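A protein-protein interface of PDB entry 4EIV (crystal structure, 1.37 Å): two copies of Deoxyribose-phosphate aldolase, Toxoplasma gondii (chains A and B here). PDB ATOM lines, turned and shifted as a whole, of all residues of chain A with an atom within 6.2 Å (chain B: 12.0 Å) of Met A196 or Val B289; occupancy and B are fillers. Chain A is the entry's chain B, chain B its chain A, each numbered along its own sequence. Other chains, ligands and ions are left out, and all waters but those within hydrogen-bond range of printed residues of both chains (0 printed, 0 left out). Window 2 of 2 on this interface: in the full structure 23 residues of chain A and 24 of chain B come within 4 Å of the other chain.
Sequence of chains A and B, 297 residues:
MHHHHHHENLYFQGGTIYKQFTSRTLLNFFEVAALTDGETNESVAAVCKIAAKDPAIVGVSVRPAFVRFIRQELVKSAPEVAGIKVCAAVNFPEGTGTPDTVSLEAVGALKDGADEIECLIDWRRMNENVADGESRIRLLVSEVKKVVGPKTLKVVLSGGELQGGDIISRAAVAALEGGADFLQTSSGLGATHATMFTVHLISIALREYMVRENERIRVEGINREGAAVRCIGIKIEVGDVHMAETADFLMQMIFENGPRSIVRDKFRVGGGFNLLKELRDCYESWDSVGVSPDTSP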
ATOM      1  N   ALA A 194      -0.853 -34.005   2.646  1.00  0.00           N
ATOM      2  CA  ALA A 194      -0.406 -33.191   1.542  1.00  0.00           C
ATOM      3  C   ALA A 194       1.027 -32.778   1.692  1.00  0.00           C
ATOM      4  O   ALA A 194       1.478 -32.487   2.795  1.00  0.00           O
ATOM      5  CB  ALA A 194      -1.245 -31.938   1.432  1.00  0.00           C
ATOM      6  N   THR A 195       1.750 -32.741   0.574  1.00  0.00           N
ATOM      7  CA  THR A 195       3.068 -32.120   0.554  1.00  0.00           C
ATOM      8  C   THR A 195       3.080 -31.122  -0.613  1.00  0.00           C
ATOM      9  O   THR A 195       2.217 -31.163  -1.486  1.00  0.00           O
ATOM     10  CB  THR A 195       4.217 -33.134   0.345  1.00  0.00           C
ATOM     11  OG1 THR A 195       4.059 -33.736  -0.949  1.00  0.00           O
ATOM     12  CG2 THR A 195       4.215 -34.206   1.460  1.00  0.00           C
ATOM     13  N   MET A 196       4.080 -30.249  -0.639  1.00  0.00           N
ATOM     14  CA  MET A 196       4.237 -29.319  -1.734  1.00  0.00           C
ATOM     15  C   MET A 196       4.270 -30.109  -3.047  1.00  0.00           C
ATOM     16  O   MET A 196       3.640 -29.748  -4.043  1.00  0.00           O
ATOM     17  CB  MET A 196       5.508 -28.503  -1.559  1.00  0.00           C
ATOM     18  CG  MET A 196       5.715 -27.496  -2.665  1.00  0.00           C
ATOM     19  SD  MET A 196       7.224 -26.580  -2.540  1.00  0.00           S
ATOM     20  CE  MET A 196       8.423 -27.897  -2.821  1.00  0.00           C
ATOM     21  N   PHE A 197       4.981 -31.229  -3.036  1.00  0.00           N
ATOM     22  CA  PHE A 197       5.105 -32.078  -4.202  1.00  0.00           C
ATOM     23  C   PHE A 197       3.770 -32.620  -4.698  1.00  0.00           C
ATOM     24  O   PHE A 197       3.430 -32.505  -5.897  1.00  0.00           O
ATOM     25  CB  PHE A 197       6.076 -33.229  -3.870  1.00  0.00           C
ATOM     26  CG  PHE A 197       6.354 -34.185  -5.002  1.00  0.00           C
ATOM     27  CD1 PHE A 197       7.074 -33.795  -6.112  1.00  0.00           C
ATOM     28  CD2 PHE A 197       5.962 -35.508  -4.901  1.00  0.00           C
ATOM     29  CE1 PHE A 197       7.359 -34.714  -7.141  1.00  0.00           C
ATOM     30  CE2 PHE A 197       6.228 -36.418  -5.912  1.00  0.00           C
ATOM     31  CZ  PHE A 197       6.926 -36.022  -7.022  1.00  0.00           C
ATOM     32  N   THR A 198       2.946 -33.166  -3.795  1.00  0.00           N
ATOM     33  CA  THR A 198       1.682 -33.725  -4.280  1.00  0.00           C
ATOM     34  C   THR A 198       0.667 -32.643  -4.660  1.00  0.00           C
ATOM     35  O   THR A 198      -0.117 -32.840  -5.595  1.00  0.00           O
ATOM     36  CB  THR A 198       1.074 -34.729  -3.298  1.00  0.00           C
ATOM     37  OG1 THR A 198       0.677 -34.067  -2.090  1.00  0.00           O
ATOM     38  CG2 THR A 198       2.074 -35.878  -2.982  1.00  0.00           C
ATOM     39  N   VAL A 199       0.677 -31.500  -3.976  1.00  0.00           N
ATOM     40  CA  VAL A 199      -0.223 -30.401  -4.353  1.00  0.00           C
ATOM     41  C   VAL A 199       0.156 -29.895  -5.752  1.00  0.00           C
ATOM     42  O   VAL A 199      -0.722 -29.614  -6.587  1.00  0.00           O
ATOM     43  CB  VAL A 199      -0.213 -29.277  -3.300  1.00  0.00           C
ATOM     44  CG1 VAL A 199      -0.901 -28.000  -3.810  1.00  0.00           C
ATOM     45  CG2 VAL A 199      -0.872 -29.755  -2.005  1.00  0.00           C
ATOM     46  N   HIS A 200       1.453 -29.860  -6.048  1.00  0.00           N
ATOM     47  CA  HIS A 200       1.923 -29.445  -7.371  1.00  0.00           C
ATOM     48  C   HIS A 200       1.437 -30.422  -8.438  1.00  0.00           C
ATOM     49  O   HIS A 200       0.909 -30.033  -9.473  1.00  0.00           O
ATOM     50  CB  HIS A 200       3.458 -29.353  -7.353  1.00  0.00           C
ATOM     51  CG  HIS A 200       4.070 -29.065  -8.680  1.00  0.00           C
ATOM     52  ND1 HIS A 200       3.895 -27.871  -9.334  1.00  0.00           N
ATOM     53  CD2 HIS A 200       4.882 -29.807  -9.470  1.00  0.00           C
ATOM     54  CE1 HIS A 200       4.562 -27.891 -10.473  1.00  0.00           C
ATOM     55  NE2 HIS A 200       5.174 -29.050 -10.576  1.00  0.00           N
ATOM     56  N   LEU A 201       1.614 -31.710  -8.181  1.00  0.00           N
ATOM     57  CA  LEU A 201       1.192 -32.713  -9.161  1.00  0.00           C
ATOM     58  C   LEU A 201      -0.312 -32.731  -9.396  1.00  0.00           C
ATOM     59  O   LEU A 201      -0.776 -32.880 -10.523  1.00  0.00           O
ATOM     60  CB  LEU A 201       1.649 -34.108  -8.719  1.00  0.00           C
ATOM     61  CG  LEU A 201       3.147 -34.312  -8.763  1.00  0.00           C
ATOM     62  CD1 LEU A 201       3.445 -35.674  -8.157  1.00  0.00           C
ATOM     63  CD2 LEU A 201       3.713 -34.199 -10.179  1.00  0.00           C
ATOM     64  N   ASP A 248       1.498 -21.950   4.345  1.00  0.00           N
ATOM     65  CA  ASP A 248       2.315 -22.141   3.151  1.00  0.00           C
ATOM     66  C   ASP A 248       1.508 -22.850   2.055  1.00  0.00           C
ATOM     67  O   ASP A 248       1.643 -22.511   0.874  1.00  0.00           O
ATOM     68  CB  ASP A 248       3.606 -22.884   3.443  1.00  0.00           C
ATOM     69  CG  ASP A 248       4.572 -22.804   2.282  1.00  0.00           C
ATOM     70  OD1 ASP A 248       5.210 -21.741   2.103  1.00  0.00           O
ATOM     71  OD2 ASP A 248       4.688 -23.802   1.551  1.00  0.00           O
ATOM     72  N   PHE A 249       0.653 -23.801   2.427  1.00  0.00           N
ATOM     73  CA  PHE A 249      -0.178 -24.466   1.429  1.00  0.00           C
ATOM     74  C   PHE A 249      -1.116 -23.472   0.784  1.00  0.00           C
ATOM     75  O   PHE A 249      -1.468 -23.603  -0.385  1.00  0.00           O
ATOM     76  CB  PHE A 249      -0.956 -25.642   2.021  1.00  0.00           C
ATOM     77  CG  PHE A 249      -0.130 -26.867   2.260  1.00  0.00           C
ATOM     78  CD1 PHE A 249       0.414 -27.572   1.206  1.00  0.00           C
ATOM     79  CD2 PHE A 249       0.154 -27.296   3.549  1.00  0.00           C
ATOM     80  CE1 PHE A 249       1.182 -28.701   1.433  1.00  0.00           C
ATOM     81  CE2 PHE A 249       0.907 -28.420   3.766  1.00  0.00           C
ATOM     82  CZ  PHE A 249       1.433 -29.120   2.704  1.00  0.00           C
ATOM     83  N   GLN A 252       0.900 -21.825  -1.741  1.00  0.00           N
ATOM     84  CA  GLN A 252       1.090 -22.742  -2.868  1.00  0.00           C
ATOM     85  C   GLN A 252      -0.115 -22.729  -3.792  1.00  0.00           C
ATOM     86  O   GLN A 252       0.040 -22.621  -5.008  1.00  0.00           O
ATOM     87  CB  GLN A 252       1.333 -24.168  -2.374  1.00  0.00           C
ATOM     88  CG  GLN A 252       2.622 -24.353  -1.584  1.00  0.00           C
ATOM     89  CD  GLN A 252       2.723 -25.747  -0.984  1.00  0.00           C
ATOM     90  OE1 GLN A 252       2.146 -26.696  -1.506  1.00  0.00           O
ATOM     91  NE2 GLN A 252       3.475 -25.872   0.107  1.00  0.00           N
ATOM     92  N   PHE A 255      -0.198 -19.630  -5.877  1.00  0.00           N
ATOM     93  CA  PHE A 255       0.889 -19.679  -6.848  1.00  0.00           C
ATOM     94  C   PHE A 255       0.574 -20.628  -8.014  1.00  0.00           C
ATOM     95  O   PHE A 255       0.773 -20.293  -9.191  1.00  0.00           O
ATOM     96  CB  PHE A 255       2.177 -20.100  -6.127  1.00  0.00           C
ATOM     97  CG  PHE A 255       3.327 -20.326  -7.052  1.00  0.00           C
ATOM     98  CD1 PHE A 255       3.952 -19.258  -7.678  1.00  0.00           C
ATOM     99  CD2 PHE A 255       3.774 -21.610  -7.334  1.00  0.00           C
ATOM    100  CE1 PHE A 255       5.009 -19.472  -8.555  1.00  0.00           C
ATOM    101  CE2 PHE A 255       4.823 -21.812  -8.211  1.00  0.00           C
ATOM    102  CZ  PHE A 255       5.435 -20.746  -8.803  1.00  0.00           C
ATOM    103  N   GLU A 256       0.084 -21.820  -7.696  1.00  0.00           N
ATOM    104  CA  GLU A 256      -0.239 -22.794  -8.748  1.00  0.00           C
ATOM    105  C   GLU A 256      -1.478 -22.486  -9.541  1.00  0.00           C
ATOM    106  O   GLU A 256      -1.490 -22.627 -10.763  1.00  0.00           O
ATOM    107  CB  GLU A 256      -0.494 -24.177  -8.142  1.00  0.00           C
ATOM    108  CG  GLU A 256       0.727 -24.905  -7.607  1.00  0.00           C
ATOM    109  CD  GLU A 256       1.657 -25.457  -8.705  1.00  0.00           C
ATOM    110  OE1 GLU A 256       2.803 -25.755  -8.374  1.00  0.00           O
ATOM    111  OE2 GLU A 256       1.253 -25.575  -9.881  1.00  0.00           O
ATOM    112  N   ILE B  17       5.496 -15.914   6.598  1.00  0.00           N
ATOM    113  CA  ILE B  17       4.490 -16.399   5.668  1.00  0.00           C
ATOM    114  C   ILE B  17       3.193 -15.554   5.694  1.00  0.00           C
ATOM    115  O   ILE B  17       2.522 -15.406   4.685  1.00  0.00           O
ATOM    116  CB  ILE B  17       4.218 -17.907   5.946  1.00  0.00           C
ATOM    117  CG1 ILE B  17       3.325 -18.517   4.850  1.00  0.00           C
ATOM    118  CG2 ILE B  17       3.616 -18.134   7.344  1.00  0.00           C
ATOM    119  CD1 ILE B  17       3.865 -18.434   3.455  1.00  0.00           C
ATOM    120  N   GLN B  20       3.748 -12.394   3.743  1.00  0.00           N
ATOM    121  CA  GLN B  20       3.818 -12.794   2.337  1.00  0.00           C
ATOM    122  C   GLN B  20       2.441 -13.077   1.759  1.00  0.00           C
ATOM    123  O   GLN B  20       2.144 -12.627   0.655  1.00  0.00           O
ATOM    124  CB  GLN B  20       4.750 -13.995   2.176  1.00  0.00           C
ATOM    125  CG  GLN B  20       6.213 -13.655   2.469  1.00  0.00           C
ATOM    126  CD  GLN B  20       7.074 -14.861   2.809  1.00  0.00           C
ATOM    127  OE1 GLN B  20       6.577 -15.953   3.057  1.00  0.00           O
ATOM    128  NE2 GLN B  20       8.386 -14.652   2.812  1.00  0.00           N
ATOM    129  N   TYR B 283       6.199 -10.043  -1.105  1.00  0.00           N
ATOM    130  CA  TYR B 283       5.823 -11.255  -1.808  1.00  0.00           C
ATOM    131  C   TYR B 283       7.006 -11.999  -2.413  1.00  0.00           C
ATOM    132  O   TYR B 283       7.094 -13.238  -2.321  1.00  0.00           O
ATOM    133  CB  TYR B 283       4.802 -10.980  -2.908  1.00  0.00           C
ATOM    134  CG  TYR B 283       4.614 -12.189  -3.770  1.00  0.00           C
ATOM    135  CD1 TYR B 283       4.006 -13.329  -3.260  1.00  0.00           C
ATOM    136  CD2 TYR B 283       5.112 -12.231  -5.074  1.00  0.00           C
ATOM    137  CE1 TYR B 283       3.872 -14.473  -4.022  1.00  0.00           C
ATOM    138  CE2 TYR B 283       4.978 -13.377  -5.854  1.00  0.00           C
ATOM    139  CZ  TYR B 283       4.356 -14.496  -5.315  1.00  0.00           C
ATOM    140  OH  TYR B 283       4.186 -15.623  -6.068  1.00  0.00           O
ATOM    141  N   GLU B 284       7.937 -11.245  -2.992  1.00  0.00           N
ATOM    142  CA  GLU B 284       9.102 -11.853  -3.631  1.00  0.00           C
ATOM    143  C   GLU B 284      10.030 -12.573  -2.656  1.00  0.00           C
ATOM    144  O   GLU B 284      10.884 -13.333  -3.084  1.00  0.00           O
ATOM    145  CB  GLU B 284       9.847 -10.821  -4.485  1.00  0.00           C
ATOM    146  CG  GLU B 284       9.057 -10.463  -5.743  1.00  0.00           C
ATOM    147  CD  GLU B 284       9.676  -9.361  -6.568  1.00  0.00           C
ATOM    148  OE1 GLU B 284      10.738  -8.829  -6.169  1.00  0.00           O
ATOM    149  OE2 GLU B 284       9.095  -9.033  -7.631  1.00  0.00           O
ATOM    150  N   SER B 285       9.867 -12.352  -1.356  1.00  0.00           N
ATOM    151  CA  SER B 285      10.657 -13.082  -0.369  1.00  0.00           C
ATOM    152  C   SER B 285      10.136 -14.512  -0.122  1.00  0.00           C
ATOM    153  O   SER B 285      10.817 -15.312   0.515  1.00  0.00           O
ATOM    154  CB  SER B 285      10.767 -12.307   0.946  1.00  0.00           C
ATOM    155  OG  SER B 285       9.547 -12.211   1.649  1.00  0.00           O
ATOM    156  N   TRP B 286       8.941 -14.836  -0.619  1.00  0.00           N
ATOM    157  CA  TRP B 286       8.394 -16.182  -0.478  1.00  0.00           C
ATOM    158  C   TRP B 286       9.067 -17.147  -1.473  1.00  0.00           C
ATOM    159  O   TRP B 286       9.232 -16.813  -2.646  1.00  0.00           O
ATOM    160  CB  TRP B 286       6.874 -16.151  -0.706  1.00  0.00           C
ATOM    161  CG  TRP B 286       6.234 -17.501  -0.638  1.00  0.00           C
ATOM    162  CD1 TRP B 286       6.050 -18.268   0.479  1.00  0.00           C
ATOM    163  CD2 TRP B 286       5.696 -18.254  -1.731  1.00  0.00           C
ATOM    164  NE1 TRP B 286       5.439 -19.451   0.148  1.00  0.00           N
ATOM    165  CE2 TRP B 286       5.217 -19.474  -1.201  1.00  0.00           C
ATOM    166  CE3 TRP B 286       5.586 -18.029  -3.108  1.00  0.00           C
ATOM    167  CZ2 TRP B 286       4.619 -20.453  -1.999  1.00  0.00           C
ATOM    168  CZ3 TRP B 286       4.992 -19.007  -3.892  1.00  0.00           C
ATOM    169  CH2 TRP B 286       4.523 -20.202  -3.334  1.00  0.00           C
ATOM    170  N   ASP B 287       9.443 -18.337  -1.000  1.00  0.00           N
ATOM    171  CA  ASP B 287      10.099 -19.357  -1.839  1.00  0.00           C
ATOM    172  C   ASP B 287       9.051 -20.258  -2.503  1.00  0.00           C
ATOM    173  O   ASP B 287       8.380 -21.051  -1.832  1.00  0.00           O
ATOM    174  CB  ASP B 287      11.059 -20.195  -0.974  1.00  0.00           C
ATOM    175  CG  ASP B 287      11.880 -21.205  -1.781  1.00  0.00           C
ATOM    176  OD1 ASP B 287      11.828 -21.205  -3.035  1.00  0.00           O
ATOM    177  OD2 ASP B 287      12.598 -22.001  -1.136  1.00  0.00           O
ATOM    178  N   SER B 288       8.914 -20.133  -3.824  1.00  0.00           N
ATOM    179  CA  SER B 288       7.949 -20.923  -4.594  1.00  0.00           C
ATOM    180  C   SER B 288       8.454 -22.314  -4.953  1.00  0.00           C
ATOM    181  O   SER B 288       7.662 -23.174  -5.360  1.00  0.00           O
ATOM    182  CB  SER B 288       7.634 -20.223  -5.918  1.00  0.00           C
ATOM    183  OG  SER B 288       8.703 -20.392  -6.851  1.00  0.00           O
ATOM    184  N   VAL B 289       9.766 -22.524  -4.833  1.00  0.00           N
ATOM    185  CA  VAL B 289      10.387 -23.783  -5.245  1.00  0.00           C
ATOM    186  C   VAL B 289      10.212 -24.865  -4.178  1.00  0.00           C
ATOM    187  O   VAL B 289      10.802 -24.789  -3.098  1.00  0.00           O
ATOM    188  CB  VAL B 289      11.896 -23.586  -5.583  1.00  0.00           C
ATOM    189  CG1 VAL B 289      12.492 -24.877  -6.127  1.00  0.00           C
ATOM    190  CG2 VAL B 289      12.083 -22.447  -6.599  1.00  0.00           C
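Val B289 touches Met A196. Ile B17 touches Asp A248 (CD1 to OD1, 3.8 Å). Gln A252 touches Trp B286 (N to CZ2, 3.97 Å). Phe A255 touches Tyr B283. Phe A255 touches Trp B286. Ser B288 touches Phe A255.
No position is printed for both chains.
The backbone NH (N) of Val B289 lies within hydrogen-bond range of the side-chain carboxylate (OD1) of Asp B287 (3.0 Å). The backbone NH (N) of Trp B286 lies close to the side-chain amide nitrogen (NE2) of Gln B20 (3.5 Å). The side-chain amide nitrogen of Gln A252 sits at hydrogen-bond distance from the side-chain carboxylate of Asp A248, at 2.8 Å.
NE1 of Trp B286 is in hydrogen-bond range of OD1 of Asp A248, at 3.0 Å.
No residue of chain B comes within 4 Å of Ala A194. No residue of chain B comes within 4 Å of Thr A195. Of the printed residues of chain B, Met A196 touches Val B289. No residue of chain B comes within 4 Å of Phe A197. No residue of chain B comes within 4 Å of Thr A198. No residue of chain B comes within 4 Å of Val A199. No residue of chain B comes within 4 Å of His A200. Leu A201 touches none of the printed residues of chain B. Of the printed residues of chain B, Gln A252 touches Trp B286 (3.97 Å). Printed residues of chain A within 4 Å of Ile B17: Asp A248. Of the printed residues of chain A, Tyr B283 touches Phe A255. Printed residues of chain A within 4 Å of Val B289: Met A196 (3.8 Å). The nearest residue of chain A that does not touch Val B289 is Phe A255 (6.0 Å).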
